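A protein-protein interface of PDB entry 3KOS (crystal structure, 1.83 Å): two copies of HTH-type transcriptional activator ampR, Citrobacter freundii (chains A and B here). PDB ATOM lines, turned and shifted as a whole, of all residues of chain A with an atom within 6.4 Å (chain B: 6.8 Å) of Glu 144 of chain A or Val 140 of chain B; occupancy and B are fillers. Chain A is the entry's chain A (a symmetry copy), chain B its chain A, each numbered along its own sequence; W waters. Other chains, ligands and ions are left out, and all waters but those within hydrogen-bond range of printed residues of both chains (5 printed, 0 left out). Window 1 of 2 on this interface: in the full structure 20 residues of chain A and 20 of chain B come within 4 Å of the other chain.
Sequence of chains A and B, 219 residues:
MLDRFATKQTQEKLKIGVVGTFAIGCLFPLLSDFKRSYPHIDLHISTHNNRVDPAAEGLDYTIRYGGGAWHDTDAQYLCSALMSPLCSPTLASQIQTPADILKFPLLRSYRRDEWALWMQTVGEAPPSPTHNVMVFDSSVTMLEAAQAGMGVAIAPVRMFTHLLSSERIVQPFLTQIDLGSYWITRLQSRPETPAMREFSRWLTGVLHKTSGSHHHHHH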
ATOM      1  N   ILE A  24       7.199  25.261  -5.497  1.00  0.00           N
ATOM      2  CA  ILE A  24       5.838  25.496  -5.968  1.00  0.00           C
ATOM      3  C   ILE A  24       4.799  24.847  -5.051  1.00  0.00           C
ATOM      4  O   ILE A  24       3.754  25.432  -4.751  1.00  0.00           O
ATOM      5  CB  ILE A  24       5.645  24.947  -7.407  1.00  0.00           C
ATOM      6  CG1 ILE A  24       6.572  25.663  -8.388  1.00  0.00           C
ATOM      7  CG2 ILE A  24       4.202  25.100  -7.846  1.00  0.00           C
ATOM      8  CD1 ILE A  24       6.434  27.202  -8.386  1.00  0.00           C
ATOM      9  N   SER A 139       9.385  17.155 -11.349  1.00  0.00           N
ATOM     10  CA  SER A 139       7.980  16.748 -11.284  1.00  0.00           C
ATOM     11  C   SER A 139       7.060  17.859 -11.743  1.00  0.00           C
ATOM     12  O   SER A 139       5.930  17.594 -12.164  1.00  0.00           O
ATOM     13  CB  SER A 139       7.592  16.355  -9.848  1.00  0.00           C
ATOM     14  OG  SER A 139       8.101  15.074  -9.535  1.00  0.00           O
ATOM     15  N   VAL A 140       7.508  19.107 -11.608  1.00  0.00           N
ATOM     16  CA  VAL A 140       6.672  20.226 -12.035  1.00  0.00           C
ATOM     17  C   VAL A 140       6.414  20.074 -13.534  1.00  0.00           C
ATOM     18  O   VAL A 140       5.276  20.143 -14.000  1.00  0.00           O
ATOM     19  CB  VAL A 140       7.344  21.583 -11.767  1.00  0.00           C
ATOM     20  CG1 VAL A 140       6.510  22.705 -12.345  1.00  0.00           C
ATOM     21  CG2 VAL A 140       7.525  21.790 -10.257  1.00  0.00           C
ATOM     22  N   THR A 141       7.492  19.855 -14.277  1.00  0.00           N
ATOM     23  CA  THR A 141       7.391  19.651 -15.727  1.00  0.00           C
ATOM     24  C   THR A 141       6.596  18.384 -16.038  1.00  0.00           C
ATOM     25  O   THR A 141       5.748  18.367 -16.938  1.00  0.00           O
ATOM     26  CB  THR A 141       8.799  19.547 -16.342  1.00  0.00           C
ATOM     27  OG1 THR A 141       9.529  20.743 -16.031  1.00  0.00           O
ATOM     28  CG2 THR A 141       8.725  19.369 -17.869  1.00  0.00           C
ATOM     29  N   MET A 142       6.853  17.320 -15.289  1.00  0.00           N
ATOM     30  CA  MET A 142       6.119  16.071 -15.502  1.00  0.00           C
ATOM     31  C   MET A 142       4.602  16.279 -15.385  1.00  0.00           C
ATOM     32  O   MET A 142       3.829  15.730 -16.177  1.00  0.00           O
ATOM     33  CB  MET A 142       6.559  15.010 -14.488  1.00  0.00           C
ATOM     34  CG  MET A 142       5.834  13.710 -14.665  1.00  0.00           C
ATOM     35  SD  MET A 142       6.152  12.499 -13.138  1.00  0.00           S
ATOM     36  CE  MET A 142       8.111  12.427 -13.160  1.00  0.00           C
ATOM     37  N   LEU A 143       4.176  17.049 -14.384  1.00  0.00           N
ATOM     38  CA  LEU A 143       2.737  17.243 -14.145  1.00  0.00           C
ATOM     39  C   LEU A 143       2.094  18.168 -15.171  1.00  0.00           C
ATOM     40  O   LEU A 143       0.886  18.097 -15.407  1.00  0.00           O
ATOM     41  CB  LEU A 143       2.455  17.736 -12.718  1.00  0.00           C
ATOM     42  CG  LEU A 143       2.146  16.623 -11.707  1.00  0.00           C
ATOM     43  CD1 LEU A 143       0.809  15.960 -12.006  1.00  0.00           C
ATOM     44  CD2 LEU A 143       3.267  15.574 -11.661  1.00  0.00           C
ATOM     45  N   GLU A 144       2.892  19.039 -15.781  1.00  0.00           N
ATOM     46  CA  GLU A 144       2.398  19.803 -16.919  1.00  0.00           C
ATOM     47  C   GLU A 144       2.083  18.854 -18.061  1.00  0.00           C
ATOM     48  O   GLU A 144       1.029  18.958 -18.694  1.00  0.00           O
ATOM     49  CB  GLU A 144       3.397  20.882 -17.365  1.00  0.00           C
ATOM     50  CG  GLU A 144       3.513  22.034 -16.387  1.00  0.00           C
ATOM     51  CD  GLU A 144       2.178  22.744 -16.172  1.00  0.00           C
ATOM     52  OE1 GLU A 144       1.685  22.759 -15.019  1.00  0.00           O
ATOM     53  OE2 GLU A 144       1.620  23.271 -17.162  1.00  0.00           O
ATOM     54  N   ALA A 145       2.997  17.920 -18.324  1.00  0.00           N
ATOM     55  CA  ALA A 145       2.774  16.931 -19.380  1.00  0.00           C
ATOM     56  C   ALA A 145       1.565  16.054 -19.056  1.00  0.00           C
ATOM     57  O   ALA A 145       0.769  15.738 -19.940  1.00  0.00           O
ATOM     58  CB  ALA A 145       4.018  16.069 -19.579  1.00  0.00           C
ATOM     59  N   ALA A 146       1.429  15.661 -17.789  1.00  0.00           N
ATOM     60  CA  ALA A 146       0.276  14.869 -17.355  1.00  0.00           C
ATOM     61  C   ALA A 146      -1.049  15.624 -17.509  1.00  0.00           C
ATOM     62  O   ALA A 146      -2.053  15.044 -17.938  1.00  0.00           O
ATOM     63  CB  ALA A 146       0.457  14.382 -15.911  1.00  0.00           C
ATOM     64  N   GLN A 147      -1.066  16.909 -17.167  1.00  0.00           N
ATOM     65  CA  GLN A 147      -2.291  17.694 -17.352  1.00  0.00           C
ATOM     66  C   GLN A 147      -2.699  17.721 -18.815  1.00  0.00           C
ATOM     67  O   GLN A 147      -3.891  17.771 -19.130  1.00  0.00           O
ATOM     68  CB  GLN A 147      -2.120  19.124 -16.860  1.00  0.00           C
ATOM     69  CG  GLN A 147      -2.018  19.270 -15.360  1.00  0.00           C
ATOM     70  CD  GLN A 147      -1.647  20.674 -14.990  1.00  0.00           C
ATOM     71  OE1 GLN A 147      -2.464  21.590 -15.090  1.00  0.00           O
ATOM     72  NE2 GLN A 147      -0.401  20.865 -14.582  1.00  0.00           N
ATOM     73  N   ALA A 148      -1.713  17.684 -19.709  1.00  0.00           N
ATOM     74  CA  ALA A 148      -1.966  17.715 -21.152  1.00  0.00           C
ATOM     75  C   ALA A 148      -2.401  16.362 -21.689  1.00  0.00           C
ATOM     76  O   ALA A 148      -2.685  16.219 -22.882  1.00  0.00           O
ATOM     77  CB  ALA A 148      -0.722  18.200 -21.909  1.00  0.00           C
ATOM     78  N   GLY A 149      -2.431  15.362 -20.814  1.00  0.00           N
ATOM     79  CA  GLY A 149      -2.780  14.011 -21.215  1.00  0.00           C
ATOM     80  C   GLY A 149      -1.690  13.250 -21.950  1.00  0.00           C
ATOM     81  O   GLY A 149      -1.993  12.323 -22.704  1.00  0.00           O
ATOM     82  N   MET A 150      -0.427  13.614 -21.739  1.00  0.00           N
ATOM     83  CA  MET A 150       0.668  12.934 -22.429  1.00  0.00           C
ATOM     84  C   MET A 150       0.880  11.513 -21.883  1.00  0.00           C
ATOM     85  O   MET A 150       1.445  10.656 -22.552  1.00  0.00           O
ATOM     86  CB  MET A 150       1.980  13.735 -22.348  1.00  0.00           C
ATOM     87  CG  MET A 150       1.935  15.120 -22.995  1.00  0.00           C
ATOM     88  SD  MET A 150       1.575  14.957 -24.929  1.00  0.00           S
ATOM     89  CE  MET A 150       3.211  14.019 -25.421  1.00  0.00           C
ATOM     90  N   LEU A 163      -3.129  21.349  -8.042  1.00  0.00           N
ATOM     91  CA  LEU A 163      -3.698  20.703  -9.227  1.00  0.00           C
ATOM     92  C   LEU A 163      -4.861  19.777  -8.879  1.00  0.00           C
ATOM     93  O   LEU A 163      -5.815  19.671  -9.640  1.00  0.00           O
ATOM     94  CB  LEU A 163      -2.633  19.911  -9.995  1.00  0.00           C
ATOM     95  CG  LEU A 163      -1.412  20.696 -10.483  1.00  0.00           C
ATOM     96  CD1 LEU A 163      -0.434  19.774 -11.230  1.00  0.00           C
ATOM     97  CD2 LEU A 163      -1.843  21.866 -11.365  1.00  0.00           C
ATOM     98  N   VAL B  19      15.046  20.714 -23.122  1.00  0.00           N
ATOM     99  CA  VAL B  19      14.773  21.659 -22.034  1.00  0.00           C
ATOM    100  C   VAL B  19      13.261  21.660 -21.769  1.00  0.00           C
ATOM    101  O   VAL B  19      12.459  21.686 -22.702  1.00  0.00           O
ATOM    102  CB  VAL B  19      15.329  23.081 -22.335  1.00  0.00           C
ATOM    103  CG1 VAL B  19      14.750  23.654 -23.653  1.00  0.00           C
ATOM    104  CG2 VAL B  19      15.069  24.020 -21.168  1.00  0.00           C
ATOM    105  N   GLY B  20      12.874  21.597 -20.494  1.00  0.00           N
ATOM    106  CA  GLY B  20      11.492  21.321 -20.150  1.00  0.00           C
ATOM    107  C   GLY B  20      10.521  22.314 -20.752  1.00  0.00           C
ATOM    108  O   GLY B  20       9.423  21.955 -21.196  1.00  0.00           O
ATOM    109  N   THR B  21      10.926  23.579 -20.758  1.00  0.00           N
ATOM    110  CA  THR B  21      10.080  24.643 -21.274  1.00  0.00           C
ATOM    111  C   THR B  21       9.685  24.376 -22.724  1.00  0.00           C
ATOM    112  O   THR B  21       8.527  24.556 -23.113  1.00  0.00           O
ATOM    113  CB  THR B  21      10.776  25.998 -21.138  1.00  0.00           C
ATOM    114  OG1 THR B  21      11.007  26.258 -19.741  1.00  0.00           O
ATOM    115  CG2 THR B  21       9.908  27.108 -21.714  1.00  0.00           C
ATOM    116  N   PHE B  22      10.649  23.940 -23.520  1.00  0.00           N
ATOM    117  CA  PHE B  22      10.380  23.598 -24.925  1.00  0.00           C
ATOM    118  C   PHE B  22       9.540  22.334 -25.068  1.00  0.00           C
ATOM    119  O   PHE B  22       8.699  22.251 -25.959  1.00  0.00           O
ATOM    120  CB  PHE B  22      11.683  23.439 -25.693  1.00  0.00           C
ATOM    121  CG  PHE B  22      11.507  23.281 -27.187  1.00  0.00           C
ATOM    122  CD1 PHE B  22      11.406  22.025 -27.750  1.00  0.00           C
ATOM    123  CD2 PHE B  22      11.471  24.392 -28.020  1.00  0.00           C
ATOM    124  CE1 PHE B  22      11.266  21.870 -29.123  1.00  0.00           C
ATOM    125  CE2 PHE B  22      11.326  24.246 -29.398  1.00  0.00           C
ATOM    126  CZ  PHE B  22      11.221  22.981 -29.946  1.00  0.00           C
ATOM    127  N   ILE B  24       7.229  21.191 -23.006  1.00  0.00           N
ATOM    128  CA  ILE B  24       5.842  21.492 -22.664  1.00  0.00           C
ATOM    129  C   ILE B  24       5.209  22.467 -23.660  1.00  0.00           C
ATOM    130  O   ILE B  24       4.054  22.312 -24.064  1.00  0.00           O
ATOM    131  CB  ILE B  24       5.740  22.099 -21.239  1.00  0.00           C
ATOM    132  CG1 ILE B  24       6.238  21.105 -20.191  1.00  0.00           C
ATOM    133  CG2 ILE B  24       4.312  22.506 -20.936  1.00  0.00           C
ATOM    134  CD1 ILE B  24       5.533  19.730 -20.234  1.00  0.00           C
ATOM    135  N   GLY B  25       5.974  23.474 -24.063  1.00  0.00           N
ATOM    136  CA  GLY B  25       5.410  24.571 -24.826  1.00  0.00           C
ATOM    137  C   GLY B  25       5.405  24.364 -26.324  1.00  0.00           C
ATOM    138  O   GLY B  25       4.725  25.092 -27.042  1.00  0.00           O
ATOM    139  N   PHE B  28       5.949  18.491 -27.162  1.00  0.00           N
ATOM    140  CA  PHE B  28       5.012  17.442 -26.775  1.00  0.00           C
ATOM    141  C   PHE B  28       3.722  17.466 -27.597  1.00  0.00           C
ATOM    142  O   PHE B  28       3.257  16.419 -28.040  1.00  0.00           O
ATOM    143  CB  PHE B  28       4.718  17.477 -25.265  1.00  0.00           C
ATOM    144  CG  PHE B  28       5.825  16.910 -24.414  1.00  0.00           C
ATOM    145  CD1 PHE B  28       6.928  16.311 -24.991  1.00  0.00           C
ATOM    146  CD2 PHE B  28       5.751  16.971 -23.023  1.00  0.00           C
ATOM    147  CE1 PHE B  28       7.950  15.784 -24.199  1.00  0.00           C
ATOM    148  CE2 PHE B  28       6.755  16.447 -22.235  1.00  0.00           C
ATOM    149  CZ  PHE B  28       7.854  15.858 -22.814  1.00  0.00           C
ATOM    150  N   PHE B 136      14.894  31.366 -11.156  1.00  0.00           N
ATOM    151  CA  PHE B 136      14.397  30.056 -11.571  1.00  0.00           C
ATOM    152  C   PHE B 136      15.265  29.350 -12.608  1.00  0.00           C
ATOM    153  O   PHE B 136      15.692  29.961 -13.583  1.00  0.00           O
ATOM    154  CB  PHE B 136      12.983  30.196 -12.137  1.00  0.00           C
ATOM    155  CG  PHE B 136      11.994  30.647 -11.121  1.00  0.00           C
ATOM    156  CD1 PHE B 136      11.269  29.719 -10.392  1.00  0.00           C
ATOM    157  CD2 PHE B 136      11.828  31.991 -10.850  1.00  0.00           C
ATOM    158  CE1 PHE B 136      10.360  30.130  -9.425  1.00  0.00           C
ATOM    159  CE2 PHE B 136      10.927  32.413  -9.873  1.00  0.00           C
ATOM    160  CZ  PHE B 136      10.199  31.484  -9.161  1.00  0.00           C
ATOM    161  N   ASP B 137      15.495  28.057 -12.392  1.00  0.00           N
ATOM    162  CA  ASP B 137      16.268  27.249 -13.327  1.00  0.00           C
ATOM    163  C   ASP B 137      15.447  26.927 -14.569  1.00  0.00           C
ATOM    164  O   ASP B 137      15.997  26.666 -15.642  1.00  0.00           O
ATOM    165  CB  ASP B 137      16.728  25.949 -12.662  1.00  0.00           C
ATOM    166  CG  ASP B 137      15.564  25.037 -12.277  1.00  0.00           C
ATOM    167  OD1 ASP B 137      14.524  25.533 -11.780  1.00  0.00           O
ATOM    168  OD2 ASP B 137      15.699  23.806 -12.449  1.00  0.00           O
ATOM    169  N   SER B 138      14.125  26.950 -14.423  1.00  0.00           N
ATOM    170  CA  SER B 138      13.241  26.560 -15.526  1.00  0.00           C
ATOM    171  C   SER B 138      12.075  27.533 -15.631  1.00  0.00           C
ATOM    172  O   SER B 138      11.473  27.875 -14.622  1.00  0.00           O
ATOM    173  CB  SER B 138      12.697  25.153 -15.276  1.00  0.00           C
ATOM    174  OG  SER B 138      11.578  24.876 -16.122  1.00  0.00           O
ATOM    175  N   SER B 139      11.757  27.986 -16.839  1.00  0.00           N
ATOM    176  CA  SER B 139      10.620  28.889 -17.024  1.00  0.00           C
ATOM    177  C   SER B 139       9.313  28.213 -16.669  1.00  0.00           C
ATOM    178  O   SER B 139       8.332  28.891 -16.347  1.00  0.00           O
ATOM    179  CB  SER B 139      10.539  29.374 -18.481  1.00  0.00           C
ATOM    180  OG  SER B 139      11.518  30.364 -18.724  1.00  0.00           O
ATOM    181  N   VAL B 140       9.269  26.886 -16.785  1.00  0.00           N
ATOM    182  CA  VAL B 140       8.040  26.171 -16.455  1.00  0.00           C
ATOM    183  C   VAL B 140       7.724  26.434 -14.983  1.00  0.00           C
ATOM    184  O   VAL B 140       6.606  26.806 -14.623  1.00  0.00           O
ATOM    185  CB  VAL B 140       8.176  24.656 -16.685  1.00  0.00           C
ATOM    186  CG1 VAL B 140       6.932  23.939 -16.204  1.00  0.00           C
ATOM    187  CG2 VAL B 140       8.401  24.369 -18.176  1.00  0.00           C
ATOM    188  N   THR B 141       8.733  26.246 -14.142  1.00  0.00           N
ATOM    189  CA  THR B 141       8.586  26.498 -12.703  1.00  0.00           C
ATOM    190  C   THR B 141       8.299  27.976 -12.444  1.00  0.00           C
ATOM    191  O   THR B 141       7.442  28.326 -11.624  1.00  0.00           O
ATOM    192  CB  THR B 141       9.868  26.078 -11.962  1.00  0.00           C
ATOM    193  OG1 THR B 141      10.121  24.690 -12.227  1.00  0.00           O
ATOM    194  CG2 THR B 141       9.728  26.297 -10.445  1.00  0.00           C
ATOM    195  N   MET B 142       9.004  28.853 -13.147  1.00  0.00           N
ATOM    196  CA  MET B 142       8.776  30.290 -12.979  1.00  0.00           C
ATOM    197  C   MET B 142       7.308  30.664 -13.237  1.00  0.00           C
ATOM    198  O   MET B 142       6.730  31.477 -12.509  1.00  0.00           O
ATOM    199  CB  MET B 142       9.671  31.090 -13.931  1.00  0.00           C
ATOM    200  CG  MET B 142       9.474  32.570 -13.797  1.00  0.00           C
ATOM    201  SD  MET B 142      10.360  33.546 -15.267  1.00  0.00           S
ATOM    202  CE  MET B 142      12.192  32.878 -15.067  1.00  0.00           C
ATOM    203  N   LEU B 143       6.717  30.093 -14.285  1.00  0.00           N
ATOM    204  CA  LEU B 143       5.338  30.449 -14.657  1.00  0.00           C
ATOM    205  C   LEU B 143       4.306  29.851 -13.710  1.00  0.00           C
ATOM    206  O   LEU B 143       3.196  30.374 -13.583  1.00  0.00           O
ATOM    207  CB  LEU B 143       5.022  30.072 -16.113  1.00  0.00           C
ATOM    208  CG  LEU B 143       5.246  31.202 -17.128  1.00  0.00           C
ATOM    209  CD1 LEU B 143       4.235  32.323 -16.939  1.00  0.00           C
ATOM    210  CD2 LEU B 143       6.679  31.753 -17.053  1.00  0.00           C
ATOM    211  N   GLU B 144       4.660  28.755 -13.045  1.00  0.00           N
ATOM    212  CA  GLU B 144       3.814  28.252 -11.971  1.00  0.00           C
ATOM    213  C   GLU B 144       3.776  29.270 -10.846  1.00  0.00           C
ATOM    214  O   GLU B 144       2.708  29.580 -10.313  1.00  0.00           O
ATOM    215  CB  GLU B 144       4.291  26.885 -11.456  1.00  0.00           C
ATOM    216  CG  GLU B 144       4.054  25.756 -12.439  1.00  0.00           C
ATOM    217  CD  GLU B 144       2.575  25.596 -12.787  1.00  0.00           C
ATOM    218  OE1 GLU B 144       2.219  25.747 -13.979  1.00  0.00           O
ATOM    219  OE2 GLU B 144       1.774  25.334 -11.860  1.00  0.00           O
ATOM    220  N   ALA B 145       4.947  29.797 -10.485  1.00  0.00           N
ATOM    221  CA  ALA B 145       5.017  30.817  -9.435  1.00  0.00           C
ATOM    222  C   ALA B 145       4.259  32.077  -9.852  1.00  0.00           C
ATOM    223  O   ALA B 145       3.564  32.684  -9.038  1.00  0.00           O
ATOM    224  CB  ALA B 145       6.469  31.152  -9.109  1.00  0.00           C
ATOM    225  N   GLN B 147       1.682  32.238 -11.986  1.00  0.00           N
ATOM    226  CA  GLN B 147       0.241  31.974 -11.926  1.00  0.00           C
ATOM    227  C   GLN B 147      -0.278  32.128 -10.507  1.00  0.00           C
ATOM    228  O   GLN B 147      -1.425  32.534 -10.302  1.00  0.00           O
ATOM    229  CB  GLN B 147      -0.094  30.576 -12.426  1.00  0.00           C
ATOM    230  CG  GLN B 147       0.082  30.376 -13.913  1.00  0.00           C
ATOM    231  CD  GLN B 147      -0.069  28.929 -14.273  1.00  0.00           C
ATOM    232  OE1 GLN B 147      -1.176  28.389 -14.264  1.00  0.00           O
ATOM    233  NE2 GLN B 147       1.046  28.277 -14.569  1.00  0.00           N
ATOM    234  N   PHE B 160       4.349  29.576 -23.740  1.00  0.00           N
ATOM    235  CA  PHE B 160       3.291  29.577 -22.731  1.00  0.00           C
ATOM    236  C   PHE B 160       1.920  29.926 -23.300  1.00  0.00           C
ATOM    237  O   PHE B 160       1.043  30.408 -22.600  1.00  0.00           O
ATOM    238  CB  PHE B 160       3.695  30.442 -21.524  1.00  0.00           C
ATOM    239  CG  PHE B 160       4.887  29.885 -20.803  1.00  0.00           C
ATOM    240  CD1 PHE B 160       4.744  28.778 -19.976  1.00  0.00           C
ATOM    241  CD2 PHE B 160       6.156  30.402 -21.018  1.00  0.00           C
ATOM    242  CE1 PHE B 160       5.846  28.210 -19.344  1.00  0.00           C
ATOM    243  CE2 PHE B 160       7.267  29.845 -20.378  1.00  0.00           C
ATOM    244  CZ  PHE B 160       7.111  28.753 -19.545  1.00  0.00           C
ATOM    245  N   HIS B 162      -0.400  27.984 -23.973  1.00  0.00           N
ATOM    246  CA  HIS B 162      -1.435  27.246 -23.243  1.00  0.00           C
ATOM    247  C   HIS B 162      -1.957  28.034 -22.028  1.00  0.00           C
ATOM    248  O   HIS B 162      -3.156  28.028 -21.746  1.00  0.00           O
ATOM    249  CB  HIS B 162      -0.960  25.839 -22.839  1.00  0.00           C
ATOM    250  CG  HIS B 162       0.282  25.826 -21.998  1.00  0.00           C
ATOM    251  ND1 HIS B 162       1.540  26.051 -22.521  1.00  0.00           N
ATOM    252  CD2 HIS B 162       0.461  25.598 -20.674  1.00  0.00           C
ATOM    253  CE1 HIS B 162       2.437  25.975 -21.552  1.00  0.00           C
ATOM    254  NE2 HIS B 162       1.808  25.704 -20.421  1.00  0.00           N
ATOM    255  N   LEU B 163      -1.062  28.737 -21.338  1.00  0.00           N
ATOM    256  CA  LEU B 163      -1.451  29.570 -20.197  1.00  0.00           C
ATOM    257  C   LEU B 163      -2.145  30.859 -20.632  1.00  0.00           C
ATOM    258  O   LEU B 163      -3.054  31.328 -19.960  1.00  0.00           O
ATOM    259  CB  LEU B 163      -0.241  29.918 -19.323  1.00  0.00           C
ATOM    260  CG  LEU B 163       0.547  28.741 -18.740  1.00  0.00           C
ATOM    261  CD1 LEU B 163       1.728  29.241 -17.892  1.00  0.00           C
ATOM    262  CD2 LEU B 163      -0.369  27.833 -17.921  1.00  0.00           C
ATOM    263  N   ARG B 168      -4.820  31.842 -17.647  1.00  0.00           N
ATOM    264  CA  ARG B 168      -4.153  31.698 -16.356  1.00  0.00           C
ATOM    265  C   ARG B 168      -2.990  32.686 -16.222  1.00  0.00           C
ATOM    266  O   ARG B 168      -2.515  32.968 -15.122  1.00  0.00           O
ATOM    267  CB  ARG B 168      -3.649  30.269 -16.192  1.00  0.00           C
ATOM    268  CG  ARG B 168      -4.774  29.250 -16.112  1.00  0.00           C
ATOM    269  CD  ARG B 168      -4.226  27.837 -16.197  1.00  0.00           C
ATOM    270  NE  ARG B 168      -5.284  26.859 -16.418  1.00  0.00           N
ATOM    271  CZ  ARG B 168      -5.068  25.578 -16.706  1.00  0.00           C
ATOM    272  NH1 ARG B 168      -3.825  25.129 -16.815  1.00  0.00           N
ATOM    273  NH2 ARG B 168      -6.095  24.751 -16.895  1.00  0.00           N
HETATM  274  O   HOH W   1       3.299  25.345 -18.164  1.00  0.00           O
HETATM  275  O   HOH W   2      -5.020  21.814 -17.220  1.00  0.00           O
HETATM  276  O   HOH W   3      -0.801  24.020 -17.690  1.00  0.00           O
HETATM  277  O   HOH W   4      -2.302  24.072 -13.870  1.00  0.00           O
HETATM  278  O   HOH W   5      10.282  22.627 -14.108  1.00  0.00           O
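The side-chain carboxylate of Glu 144 of chain A sits close to the side-chain carboxylate of Glu 144 of chain B (3.2 Å).
The side-chain hydroxyl of Thr 21 of chain B lies within hydrogen-bond range of the backbone NH of Val 140 of chain B, 3.5 Å away.
N of Val 140 of chain B lies close to OG of Ser 138 of chain B (3.1 Å).
OE1 of Glu 144 of chain B sits at hydrogen-bond distance from NE2 of Gln 147 of chain B (2.9 Å).
OE1 of Glu 144 of chain A is in hydrogen-bond range of NE2 of Gln 147 of chain A (2.9 Å).
The backbone NH (N) of Met 150 of chain A sits at hydrogen-bond distance from the backbone carbonyl oxygen (O) of Ala 145 of chain A (3.0 Å).
Ile 24 of chain A touches Thr 141 of chain B (CD1 to O, 3.6 Å).
Glu 144 of chain B touches Ile 24 of chain A.
Ala 145 of chain B touches Ile 24 of chain A (N to CD1, 3.7 Å).
CG of Glu 144 of chain B touches CG1 of Val 140 of chain A, at 3.9 Å.
CD1 of Ile 24 of chain B touches O of Thr 141 of chain A, 3.6 Å away.
CD1 of Ile 24 of chain B touches CB of Glu 144 of chain A, 3.8 Å away.
Glu 144 of chain A touches Val 140 of chain B.
Ala 145 of chain A touches Ile 24 of chain B (N to CD1, 3.7 Å).
Ala 145 of chain A touches Phe 28 of chain B.
Phe 28 of chain B touches Met 150 of chain A.
Of the printed residues of chain B, Glu 144 of chain A touches Ile 24 (3.8 Å), Val 140 (3.9 Å) and Glu 144 (3.2 Å).
Of the printed residues of chain A, Ile 24 of chain B touches Thr 141, Glu 144 and Ala 145.
Of the printed residues of chain A, Glu 144 of chain B touches Ile 24, Val 140 and Glu 144.
Of the printed residues of chain A, Ala 145 of chain B touches Ile 24.
Printed residues of chain A within 4 Å of Phe 28 of chain B: Ala 145 (3.8 Å) and Met 150 (3.6 Å).
Printed residues of chain A within 4 Å of Thr 141 of chain B: Ile 24 (3.6 Å).
Arg 168 of chain B touches none of the printed residues of chain A.
Printed residues of chain B that touch a printed residue of chain A: Ile 24, Phe 28, Val 140, Thr 141, Glu 144 and Ala 145.
Among the printed residues, no Asp or Glu carboxylate lies within 4 Å of a Lys or Arg side-chain nitrogen of the other chain.
Ile 24 of chain A touches Thr 141 of chain B, and with the chains exchanged Thr 141 of chain A touches Ile 24 of chain B.
Ile 24 of chain A touches Ala 145 of chain B, and with the chains exchanged Ala 145 of chain A touches Ile 24 of chain B.
Val 140 of chain A touches Glu 144 of chain B, and with the chains exchanged Glu 144 of chain A touches Val 140 of chain B.
Glu 144 of chain A touches its own counterpart, Glu 144 of chain B.
Of the 11 pairs that touch across the chains among the printed residues, 9 have their exchanged pair printed and touching as well.
Water W3 lies within hydrogen-bond range of OE2 of Glu 144 of chain A (2.6 Å) and NH1 of Arg 168 of chain B (3.3 Å).
Water W1 lies within hydrogen-bond range of a ring nitrogen (NE2) of His 162 of chain B (2.7 Å) and the side-chain carboxylate (OE2) of Glu 144 of chain A (2.9 Å).
Water W4 bridges OE1 of Gln 147 of chain A (2.8 Å) and NH1 of Arg 168 of chain B (3.5 Å).
Water W5 lies within hydrogen-bond range of the side-chain hydroxyl (OG1) of Thr 141 of chain A (2.8 Å), the side-chain hydroxyl (OG1) of Thr 141 of chain B (2.8 Å) and the side-chain hydroxyl (OG) of Ser 138 of chain B (3.3 Å).
Water W2 bridges NH2 of Arg 168 of chain B and OE1 of Gln 147 of chain A.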
